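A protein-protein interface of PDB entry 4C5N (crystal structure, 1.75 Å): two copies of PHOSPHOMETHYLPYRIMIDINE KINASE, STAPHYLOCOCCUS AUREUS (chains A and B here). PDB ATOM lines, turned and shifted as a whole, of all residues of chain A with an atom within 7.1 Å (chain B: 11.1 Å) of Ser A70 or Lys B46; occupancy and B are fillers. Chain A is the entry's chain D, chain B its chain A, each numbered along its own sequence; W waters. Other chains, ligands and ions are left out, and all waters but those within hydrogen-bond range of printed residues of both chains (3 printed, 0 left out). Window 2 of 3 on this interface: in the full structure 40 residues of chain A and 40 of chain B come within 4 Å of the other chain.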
ATOM      1  N   LYS A   5      10.817  19.330 -36.802  1.00  0.00           N
ATOM      2  CA  LYS A   5      10.744  19.238 -35.339  1.00  0.00           C
ATOM      3  C   LYS A   5       9.430  18.503 -35.033  1.00  0.00           C
ATOM      4  O   LYS A   5       8.354  18.967 -35.385  1.00  0.00           O
ATOM      5  CB  LYS A   5      10.797  20.599 -34.674  1.00  0.00           C
ATOM      6  CG  LYS A   5      12.126  21.324 -35.002  1.00  0.00           C
ATOM      7  CD  LYS A   5      12.025  22.801 -34.677  1.00  0.00           C
ATOM      8  CE  LYS A   5      11.282  23.479 -35.761  1.00  0.00           C
ATOM      9  NZ  LYS A   5      10.983  24.910 -35.461  1.00  0.00           N
ATOM     10  N   GLN A  64       7.456  21.719 -19.438  1.00  0.00           N
ATOM     11  CA  GLN A  64       7.914  21.017 -20.648  1.00  0.00           C
ATOM     12  C   GLN A  64       7.205  21.479 -21.905  1.00  0.00           C
ATOM     13  O   GLN A  64       7.815  21.786 -22.967  1.00  0.00           O
ATOM     14  CB  GLN A  64       7.713  19.521 -20.497  1.00  0.00           C
ATOM     15  CG  GLN A  64       8.685  18.862 -19.587  1.00  0.00           C
ATOM     16  CD  GLN A  64       8.302  17.412 -19.364  1.00  0.00           C
ATOM     17  OE1 GLN A  64       8.833  16.524 -19.971  1.00  0.00           O
ATOM     18  NE2 GLN A  64       7.324  17.186 -18.539  1.00  0.00           N
ATOM     19  N   LEU A  65       5.887  21.585 -21.775  1.00  0.00           N
ATOM     20  CA  LEU A  65       5.065  22.123 -22.870  1.00  0.00           C
ATOM     21  C   LEU A  65       5.428  23.544 -23.303  1.00  0.00           C
ATOM     22  O   LEU A  65       5.441  23.814 -24.500  1.00  0.00           O
ATOM     23  CB  LEU A  65       3.567  22.088 -22.528  1.00  0.00           C
ATOM     24  CG  LEU A  65       2.844  20.763 -22.591  1.00  0.00           C
ATOM     25  CD1 LEU A  65       1.368  21.005 -22.250  1.00  0.00           C
ATOM     26  CD2 LEU A  65       2.993  20.098 -23.958  1.00  0.00           C
ATOM     27  N   GLU A  66       5.665  24.451 -22.373  1.00  0.00           N
ATOM     28  CA  GLU A  66       6.160  25.806 -22.711  1.00  0.00           C
ATOM     29  C   GLU A  66       7.463  25.783 -23.517  1.00  0.00           C
ATOM     30  O   GLU A  66       7.637  26.467 -24.488  1.00  0.00           O
ATOM     31  CB  GLU A  66       6.419  26.604 -21.431  1.00  0.00           C
ATOM     32  CG  GLU A  66       6.994  28.022 -21.657  1.00  0.00           C
ATOM     33  CD  GLU A  66       7.216  28.811 -20.376  1.00  0.00           C
ATOM     34  OE1 GLU A  66       6.380  28.704 -19.413  1.00  0.00           O
ATOM     35  OE2 GLU A  66       8.184  29.606 -20.326  1.00  0.00           O
ATOM     36  N   THR A  67       8.383  24.950 -23.088  1.00  0.00           N
ATOM     37  CA  THR A  67       9.654  24.831 -23.786  1.00  0.00           C
ATOM     38  C   THR A  67       9.426  24.334 -25.239  1.00  0.00           C
ATOM     39  O   THR A  67       9.904  24.929 -26.218  1.00  0.00           O
ATOM     40  CB  THR A  67      10.527  23.823 -23.042  1.00  0.00           C
ATOM     41  OG1 THR A  67      10.836  24.338 -21.752  1.00  0.00           O
ATOM     42  CG2 THR A  67      11.887  23.567 -23.811  1.00  0.00           C
ATOM     43  N   ALA A  68       8.700  23.218 -25.360  1.00  0.00           N
ATOM     44  CA  ALA A  68       8.411  22.627 -26.654  1.00  0.00           C
ATOM     45  C   ALA A  68       7.667  23.588 -27.569  1.00  0.00           C
ATOM     46  O   ALA A  68       8.031  23.775 -28.737  1.00  0.00           O
ATOM     47  CB  ALA A  68       7.634  21.339 -26.475  1.00  0.00           C
ATOM     48  N   LEU A  69       6.638  24.252 -27.062  1.00  0.00           N
ATOM     49  CA  LEU A  69       5.890  25.199 -27.929  1.00  0.00           C
ATOM     50  C   LEU A  69       6.779  26.328 -28.423  1.00  0.00           C
ATOM     51  O   LEU A  69       6.652  26.823 -29.567  1.00  0.00           O
ATOM     52  CB  LEU A  69       4.686  25.746 -27.178  1.00  0.00           C
ATOM     53  CG  LEU A  69       3.835  26.815 -27.867  1.00  0.00           C
ATOM     54  CD1 LEU A  69       2.968  26.162 -28.921  1.00  0.00           C
ATOM     55  CD2 LEU A  69       2.978  27.573 -26.832  1.00  0.00           C
ATOM     56  N   SER A  70       7.620  26.815 -27.537  1.00  0.00           N
ATOM     57  CA  SER A  70       8.532  27.889 -27.878  1.00  0.00           C
ATOM     58  C   SER A  70       9.462  27.464 -29.030  1.00  0.00           C
ATOM     59  O   SER A  70       9.714  28.196 -29.968  1.00  0.00           O
ATOM     60  CB  SER A  70       9.367  28.292 -26.655  1.00  0.00           C
ATOM     61  OG  SER A  70      10.260  29.367 -26.976  1.00  0.00           O
ATOM     62  N   ILE A  71       9.992  26.262 -28.936  1.00  0.00           N
ATOM     63  CA  ILE A  71      10.801  25.737 -30.051  1.00  0.00           C
ATOM     64  C   ILE A  71      10.000  25.662 -31.352  1.00  0.00           C
ATOM     65  O   ILE A  71      10.573  25.915 -32.442  1.00  0.00           O
ATOM     66  CB  ILE A  71      11.378  24.396 -29.636  1.00  0.00           C
ATOM     67  CG1 ILE A  71      12.391  24.579 -28.474  1.00  0.00           C
ATOM     68  CG2 ILE A  71      11.945  23.676 -30.855  1.00  0.00           C
ATOM     69  CD1 ILE A  71      12.765  23.291 -27.832  1.00  0.00           C
ATOM     70  N   GLY A  72       8.687  25.324 -31.285  1.00  0.00           N
ATOM     71  CA  GLY A  72       7.817  25.332 -32.499  1.00  0.00           C
ATOM     72  C   GLY A  72       7.831  24.000 -33.244  1.00  0.00           C
ATOM     73  O   GLY A  72       8.540  23.833 -34.231  1.00  0.00           O
ATOM     74  N   PRO A  73       7.058  23.014 -32.771  1.00  0.00           N
ATOM     75  CA  PRO A  73       6.943  21.774 -33.522  1.00  0.00           C
ATOM     76  C   PRO A  73       6.278  21.962 -34.903  1.00  0.00           C
ATOM     77  O   PRO A  73       5.377  22.848 -35.089  1.00  0.00           O
ATOM     78  CB  PRO A  73       6.067  20.898 -32.580  1.00  0.00           C
ATOM     79  CG  PRO A  73       5.258  21.867 -31.838  1.00  0.00           C
ATOM     80  CD  PRO A  73       6.119  23.061 -31.633  1.00  0.00           C
ATOM     81  N   VAL A  93      -2.245  22.781 -26.711  1.00  0.00           N
ATOM     82  CA  VAL A  93      -0.910  23.116 -27.285  1.00  0.00           C
ATOM     83  C   VAL A  93      -0.799  22.888 -28.805  1.00  0.00           C
ATOM     84  O   VAL A  93      -0.120  23.644 -29.498  1.00  0.00           O
ATOM     85  CB  VAL A  93       0.310  22.498 -26.539  1.00  0.00           C
ATOM     86  CG1 VAL A  93       0.479  21.036 -26.840  1.00  0.00           C
ATOM     87  CG2 VAL A  93       1.582  23.234 -26.935  1.00  0.00           C
ATOM     88  N   THR B  14      14.553  18.952 -22.115  1.00  0.00           N
ATOM     89  CA  THR B  14      13.375  19.174 -22.932  1.00  0.00           C
ATOM     90  C   THR B  14      13.651  19.707 -24.331  1.00  0.00           C
ATOM     91  O   THR B  14      12.845  19.436 -25.266  1.00  0.00           O
ATOM     92  CB  THR B  14      12.369  20.078 -22.220  1.00  0.00           C
ATOM     93  OG1 THR B  14      12.107  19.484 -20.946  1.00  0.00           O
ATOM     94  CG2 THR B  14      11.080  20.188 -23.008  1.00  0.00           C
ATOM     95  N   SER B  15      14.723  20.470 -24.506  1.00  0.00           N
ATOM     96  CA  SER B  15      15.047  21.017 -25.816  1.00  0.00           C
ATOM     97  C   SER B  15      15.534  19.911 -26.775  1.00  0.00           C
ATOM     98  O   SER B  15      15.617  20.155 -27.994  1.00  0.00           O
ATOM     99  CB  SER B  15      16.112  22.161 -25.765  1.00  0.00           C
ATOM    100  OG  SER B  15      17.364  21.651 -25.421  1.00  0.00           O
ATOM    101  N   VAL B  42      14.742  18.830 -17.145  1.00  0.00           N
ATOM    102  CA  VAL B  42      15.233  20.189 -17.341  1.00  0.00           C
ATOM    103  C   VAL B  42      14.371  20.895 -18.385  1.00  0.00           C
ATOM    104  O   VAL B  42      14.196  20.344 -19.504  1.00  0.00           O
ATOM    105  CB  VAL B  42      16.695  20.168 -17.840  1.00  0.00           C
ATOM    106  CG1 VAL B  42      17.191  21.578 -18.026  1.00  0.00           C
ATOM    107  CG2 VAL B  42      17.601  19.455 -16.900  1.00  0.00           C
ATOM    108  N   THR B  43      13.889  22.104 -18.030  1.00  0.00           N
ATOM    109  CA  THR B  43      13.001  22.865 -18.840  1.00  0.00           C
ATOM    110  C   THR B  43      13.576  24.239 -18.960  1.00  0.00           C
ATOM    111  O   THR B  43      14.421  24.615 -18.157  1.00  0.00           O
ATOM    112  CB  THR B  43      11.597  22.904 -18.201  1.00  0.00           C
ATOM    113  OG1 THR B  43      11.670  23.495 -16.909  1.00  0.00           O
ATOM    114  CG2 THR B  43      11.043  21.464 -18.105  1.00  0.00           C
ATOM    115  N   MET B  44      13.082  25.012 -19.923  1.00  0.00           N
ATOM    116  CA  MET B  44      13.624  26.336 -20.180  1.00  0.00           C
ATOM    117  C   MET B  44      12.524  27.359 -20.424  1.00  0.00           C
ATOM    118  O   MET B  44      11.534  27.103 -21.077  1.00  0.00           O
ATOM    119  CB  MET B  44      14.464  26.300 -21.447  1.00  0.00           C
ATOM    120  CG  MET B  44      15.635  25.392 -21.367  1.00  0.00           C
ATOM    121  SD  MET B  44      15.157  23.723 -21.731  1.00  0.00           S
ATOM    122  CE  MET B  44      16.719  23.020 -21.332  1.00  0.00           C
ATOM    123  N   ASP B  45      12.731  28.541 -19.943  1.00  0.00           N
ATOM    124  CA  ASP B  45      11.732  29.569 -20.028  1.00  0.00           C
ATOM    125  C   ASP B  45      11.574  30.100 -21.449  1.00  0.00           C
ATOM    126  O   ASP B  45      12.558  30.316 -22.128  1.00  0.00           O
ATOM    127  CB  ASP B  45      12.126  30.689 -19.051  1.00  0.00           C
ATOM    128  CG  ASP B  45      11.122  31.826 -19.039  1.00  0.00           C
ATOM    129  OD1 ASP B  45      11.207  32.745 -19.905  1.00  0.00           O
ATOM    130  OD2 ASP B  45      10.206  31.746 -18.190  1.00  0.00           O
ATOM    131  N   LYS B  46      10.336  30.311 -21.902  1.00  0.00           N
ATOM    132  CA  LYS B  46      10.111  30.695 -23.314  1.00  0.00           C
ATOM    133  C   LYS B  46      10.691  32.070 -23.670  1.00  0.00           C
ATOM    134  O   LYS B  46      11.011  32.324 -24.812  1.00  0.00           O
ATOM    135  CB  LYS B  46       8.620  30.683 -23.670  1.00  0.00           C
ATOM    136  CG  LYS B  46       7.745  31.689 -22.941  1.00  0.00           C
ATOM    137  CD  LYS B  46       6.368  31.817 -23.609  1.00  0.00           C
ATOM    138  CE  LYS B  46       5.595  32.931 -22.938  1.00  0.00           C
ATOM    139  NZ  LYS B  46       5.726  34.215 -23.700  1.00  0.00           N
ATOM    140  N   ASP B  47      10.815  32.938 -22.680  1.00  0.00           N
ATOM    141  CA  ASP B  47      11.192  34.317 -22.940  1.00  0.00           C
ATOM    142  C   ASP B  47      12.672  34.520 -22.745  1.00  0.00           C
ATOM    143  O   ASP B  47      13.298  35.165 -23.591  1.00  0.00           O
ATOM    144  CB  ASP B  47      10.384  35.246 -22.058  1.00  0.00           C
ATOM    145  CG  ASP B  47       8.958  35.256 -22.442  1.00  0.00           C
ATOM    146  OD1 ASP B  47       8.703  35.294 -23.670  1.00  0.00           O
ATOM    147  OD2 ASP B  47       8.081  35.202 -21.541  1.00  0.00           O
ATOM    148  N   THR B  48      13.239  33.938 -21.680  1.00  0.00           N
ATOM    149  CA  THR B  48      14.664  34.130 -21.364  1.00  0.00           C
ATOM    150  C   THR B  48      15.517  32.906 -21.561  1.00  0.00           C
ATOM    151  O   THR B  48      16.756  33.028 -21.596  1.00  0.00           O
ATOM    152  CB  THR B  48      14.855  34.589 -19.911  1.00  0.00           C
ATOM    153  OG1 THR B  48      14.393  33.554 -19.028  1.00  0.00           O
ATOM    154  CG2 THR B  48      14.107  35.943 -19.624  1.00  0.00           C
ATOM    155  N   TRP B  49      14.879  31.731 -21.680  1.00  0.00           N
ATOM    156  CA  TRP B  49      15.550  30.450 -21.811  1.00  0.00           C
ATOM    157  C   TRP B  49      16.233  30.020 -20.505  1.00  0.00           C
ATOM    158  O   TRP B  49      17.106  29.166 -20.540  1.00  0.00           O
ATOM    159  CB  TRP B  49      16.581  30.443 -22.964  1.00  0.00           C
ATOM    160  CG  TRP B  49      16.617  29.101 -23.619  1.00  0.00           C
ATOM    161  CD1 TRP B  49      17.639  28.194 -23.633  1.00  0.00           C
ATOM    162  CD2 TRP B  49      15.546  28.507 -24.312  1.00  0.00           C
ATOM    163  NE1 TRP B  49      17.263  27.083 -24.304  1.00  0.00           N
ATOM    164  CE2 TRP B  49      15.965  27.235 -24.718  1.00  0.00           C
ATOM    165  CE3 TRP B  49      14.237  28.917 -24.594  1.00  0.00           C
ATOM    166  CZ2 TRP B  49      15.137  26.372 -25.430  1.00  0.00           C
ATOM    167  CZ3 TRP B  49      13.403  28.045 -25.303  1.00  0.00           C
ATOM    168  CH2 TRP B  49      13.885  26.776 -25.728  1.00  0.00           C
ATOM    169  N   SER B  50      15.836  30.606 -19.386  1.00  0.00           N
ATOM    170  CA  SER B  50      16.423  30.281 -18.080  1.00  0.00           C
ATOM    171  C   SER B  50      16.056  28.810 -17.802  1.00  0.00           C
ATOM    172  O   SER B  50      14.949  28.399 -18.121  1.00  0.00           O
ATOM    173  CB  SER B  50      15.857  31.247 -17.057  1.00  0.00           C
ATOM    174  OG  SER B  50      16.257  30.917 -15.775  1.00  0.00           O
ATOM    175  N   HIS B  51      17.013  28.017 -17.347  1.00  0.00           N
ATOM    176  CA  HIS B  51      16.794  26.610 -17.097  1.00  0.00           C
ATOM    177  C   HIS B  51      16.196  26.407 -15.731  1.00  0.00           C
ATOM    178  O   HIS B  51      16.566  27.104 -14.757  1.00  0.00           O
ATOM    179  CB  HIS B  51      18.126  25.838 -17.133  1.00  0.00           C
ATOM    180  CG  HIS B  51      18.746  25.767 -18.498  1.00  0.00           C
ATOM    181  ND1 HIS B  51      18.570  26.748 -19.455  1.00  0.00           N
ATOM    182  CD2 HIS B  51      19.508  24.807 -19.082  1.00  0.00           C
ATOM    183  CE1 HIS B  51      19.198  26.399 -20.565  1.00  0.00           C
ATOM    184  NE2 HIS B  51      19.788  25.234 -20.359  1.00  0.00           N
ATOM    185  N   ASP B  52      15.361  25.382 -15.623  1.00  0.00           N
ATOM    186  CA  ASP B  52      14.968  24.909 -14.320  1.00  0.00           C
ATOM    187  C   ASP B  52      15.101  23.386 -14.268  1.00  0.00           C
ATOM    188  O   ASP B  52      14.746  22.672 -15.276  1.00  0.00           O
ATOM    189  CB  ASP B  52      13.530  25.332 -14.005  1.00  0.00           C
ATOM    190  CG  ASP B  52      13.150  25.026 -12.554  1.00  0.00           C
ATOM    191  OD1 ASP B  52      13.876  25.468 -11.690  1.00  0.00           O
ATOM    192  OD2 ASP B  52      12.155  24.323 -12.325  1.00  0.00           O
ATOM    193  N   TRP B 249      22.609  23.115 -35.945  1.00  0.00           N
ATOM    194  CA  TRP B 249      21.669  24.002 -36.621  1.00  0.00           C
ATOM    195  C   TRP B 249      21.002  24.882 -35.591  1.00  0.00           C
ATOM    196  O   TRP B 249      20.914  24.489 -34.480  1.00  0.00           O
ATOM    197  CB  TRP B 249      20.573  23.226 -37.443  1.00  0.00           C
ATOM    198  CG  TRP B 249      19.790  22.206 -36.666  1.00  0.00           C
ATOM    199  CD1 TRP B 249      20.144  20.933 -36.419  1.00  0.00           C
ATOM    200  CD2 TRP B 249      18.541  22.408 -36.033  1.00  0.00           C
ATOM    201  NE1 TRP B 249      19.201  20.324 -35.634  1.00  0.00           N
ATOM    202  CE2 TRP B 249      18.175  21.194 -35.432  1.00  0.00           C
ATOM    203  CE3 TRP B 249      17.650  23.476 -35.960  1.00  0.00           C
ATOM    204  CZ2 TRP B 249      17.019  21.069 -34.668  1.00  0.00           C
ATOM    205  CZ3 TRP B 249      16.504  23.340 -35.213  1.00  0.00           C
ATOM    206  CH2 TRP B 249      16.169  22.152 -34.617  1.00  0.00           C
ATOM    207  N   LYS B 250      20.443  25.994 -36.028  1.00  0.00           N
ATOM    208  CA  LYS B 250      19.892  27.025 -35.096  1.00  0.00           C
ATOM    209  C   LYS B 250      18.475  26.691 -34.733  1.00  0.00           C
ATOM    210  O   LYS B 250      17.574  26.688 -35.620  1.00  0.00           O
ATOM    211  CB  LYS B 250      19.898  28.424 -35.757  1.00  0.00           C
ATOM    212  CG  LYS B 250      19.521  29.567 -34.824  1.00  0.00           C
ATOM    213  CD  LYS B 250      19.412  30.871 -35.633  1.00  0.00           C
ATOM    214  CE  LYS B 250      18.974  32.092 -34.805  1.00  0.00           C
ATOM    215  NZ  LYS B 250      19.553  32.086 -33.453  1.00  0.00           N
ATOM    216  N   MET B 251      18.252  26.440 -33.456  1.00  0.00           N
ATOM    217  CA  MET B 251      16.883  26.123 -32.971  1.00  0.00           C
ATOM    218  C   MET B 251      16.112  27.426 -32.682  1.00  0.00           C
ATOM    219  O   MET B 251      15.055  27.618 -33.211  1.00  0.00           O
ATOM    220  CB  MET B 251      16.952  25.166 -31.774  1.00  0.00           C
ATOM    221  CG  MET B 251      15.712  25.087 -30.847  1.00  0.00           C
ATOM    222  SD  MET B 251      15.843  23.680 -29.697  1.00  0.00           S
ATOM    223  CE  MET B 251      15.787  22.420 -30.962  1.00  0.00           C
ATOM    224  N   ASN B 252      16.716  28.348 -31.921  1.00  0.00           N
ATOM    225  CA  ASN B 252      16.144  29.648 -31.626  1.00  0.00           C
ATOM    226  C   ASN B 252      17.309  30.549 -31.206  1.00  0.00           C
ATOM    227  O   ASN B 252      18.466  30.195 -31.426  1.00  0.00           O
ATOM    228  CB  ASN B 252      15.070  29.505 -30.504  1.00  0.00           C
ATOM    229  CG  ASN B 252      15.673  29.027 -29.178  1.00  0.00           C
ATOM    230  OD1 ASN B 252      16.873  29.194 -28.927  1.00  0.00           O
ATOM    231  ND2 ASN B 252      14.836  28.502 -28.303  1.00  0.00           N
ATOM    232  N   ASP B 253      17.057  31.701 -30.583  1.00  0.00           N
ATOM    233  CA  ASP B 253      18.156  32.654 -30.403  1.00  0.00           C
ATOM    234  C   ASP B 253      19.131  32.180 -29.326  1.00  0.00           C
ATOM    235  O   ASP B 253      20.265  32.650 -29.268  1.00  0.00           O
ATOM    236  CB  ASP B 253      17.634  34.043 -30.139  1.00  0.00           C
ATOM    237  CG  ASP B 253      17.038  34.687 -31.378  1.00  0.00           C
ATOM    238  OD1 ASP B 253      17.660  34.617 -32.461  1.00  0.00           O
ATOM    239  OD2 ASP B 253      15.981  35.283 -31.257  1.00  0.00           O
ATOM    240  N   PHE B 254      18.710  31.170 -28.561  1.00  0.00           N
ATOM    241  CA  PHE B 254      19.451  30.706 -27.399  1.00  0.00           C
ATOM    242  C   PHE B 254      20.213  29.445 -27.606  1.00  0.00           C
ATOM    243  O   PHE B 254      21.157  29.179 -26.853  1.00  0.00           O
ATOM    244  CB  PHE B 254      18.480  30.424 -26.244  1.00  0.00           C
ATOM    245  CG  PHE B 254      17.683  31.617 -25.885  1.00  0.00           C
ATOM    246  CD1 PHE B 254      18.285  32.634 -25.157  1.00  0.00           C
ATOM    247  CD2 PHE B 254      16.367  31.745 -26.289  1.00  0.00           C
ATOM    248  CE1 PHE B 254      17.583  33.779 -24.843  1.00  0.00           C
ATOM    249  CE2 PHE B 254      15.638  32.888 -25.969  1.00  0.00           C
ATOM    250  CZ  PHE B 254      16.241  33.884 -25.227  1.00  0.00           C
ATOM    251  N   VAL B 255      19.779  28.640 -28.556  1.00  0.00           N
ATOM    252  CA  VAL B 255      20.271  27.285 -28.620  1.00  0.00           C
ATOM    253  C   VAL B 255      20.318  26.748 -30.040  1.00  0.00           C
ATOM    254  O   VAL B 255      19.425  27.068 -30.861  1.00  0.00           O
ATOM    255  CB  VAL B 255      19.501  26.329 -27.688  1.00  0.00           C
ATOM    256  CG1 VAL B 255      18.121  25.967 -28.200  1.00  0.00           C
ATOM    257  CG2 VAL B 255      20.358  25.103 -27.445  1.00  0.00           C
HETATM  258  O   HOH W   1       9.341  25.989 -19.288  1.00  0.00           O
HETATM  259  O   HOH W   2      12.236  29.190 -28.913  1.00  0.00           O
HETATM  260  O   HOH W   3      11.569  16.727 -20.955  1.00  0.00           O
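The backbone carbonyl oxygen of Met B44 sits at hydrogen-bond distance from the side-chain hydroxyl of Thr A67 (2.9 Å). The side-chain carboxylate (OE2) of Glu A66 sits at hydrogen-bond distance from the backbone NH (N) of Lys B46 (2.8 Å).
The side-chain amino group (NZ) of Lys A5 sits at hydrogen-bond distance from the backbone carbonyl oxygen (O) of Ile A71 (3.2 Å). The backbone NH of Thr B48 sits at hydrogen-bond distance from the side-chain carboxylate of Asp B45 (3.0 Å). OD1 of Asp B45 is in hydrogen-bond range of N of Asp B47, 2.8 Å away. The side-chain amino group (NZ) of Lys B46 is in salt-bridge range of the side-chain carboxylate (OD1) of Asp B47, 3.2 Å away. O of Val B42 is in hydrogen-bond range of OG1 of Thr B14 (2.7 Å). The backbone carbonyl oxygen (O) of Thr B43 is in hydrogen-bond range of the backbone NH (N) of Asp B52 (2.8 Å).
Gln A64 touches Thr B14 (O to CG2, 3.6 Å). Gln A64 touches Thr B43. Glu A66 touches Asp B45. Thr B14 touches Thr A67. OG1 of Thr A67 touches CB of Thr B43 (3.9 Å). Lys B46 touches Ser A70. Ser A70 touches Trp B49. CA of Ser B15 touches CD1 of Ile A71, at 3.8 Å. CG1 of Ile A71 touches CH2 of Trp B49, 3.8 Å away. CD1 of Ile A71 touches SD of Met B251, 3.6 Å away.
Ser A70 touches two residues of chain B. Of chain A, only Glu A66 (2.8 Å) and Ser A70 (3.7 Å) come within 4 Å of Lys B46. Glu A66 touches just these residues of chain B: Asp B45 (3.6 Å) and Lys B46 (2.8 Å). Of chain B, only Thr B14, Thr B43 and Met B44 come within 4 Å of Thr A67. No residue of chain B comes within 4 Å of Ala A68. Of the printed residues of chain A, Met B251 touches Ile A71. Of the printed residues of chain A, Met B44 touches Thr A67. Of the printed residues of chain A, Ser B15 touches Ile A71 (3.8 Å). Of the printed residues of chain B, Gln A64 touches Thr B14 (3.6 Å) and Thr B43 (3.8 Å). The nearest residue of chain B that does not touch Ser A70 is Asn B252 (4.8 Å). The nearest residue of chain A that does not touch Lys B46 is Thr A67 (5.8 Å). The nearest printed residue of chain A that does not touch Thr B14 is Ala A68 (4.5 Å).
Hydrophobic or aromatic side chains of chain B that line the printed part of chain A: Met B44, Trp B49 and Met B251. Hydrophobic or aromatic side chains of chain A that line the printed part of chain B: Ile A71. Among the printed residues, 12 pairs touch across the chains.
No position is printed for both chains. Of the 12 pairs that touch across the chains among the printed residues, none has its exchanged pair printed and touching as well.
Water W2 bridges the side-chain amide nitrogen (ND2) of Asn B252 and the side-chain hydroxyl (OG) of Ser A70. Water W3 lies within hydrogen-bond range of the side-chain hydroxyl (OG1) of Thr B14 (2.8 Å) and the side-chain amide oxygen (OE1) of Gln A64 (2.9 Å). Water W1 lies within hydrogen-bond range of O of Met B44 and OG1 of Thr A67.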
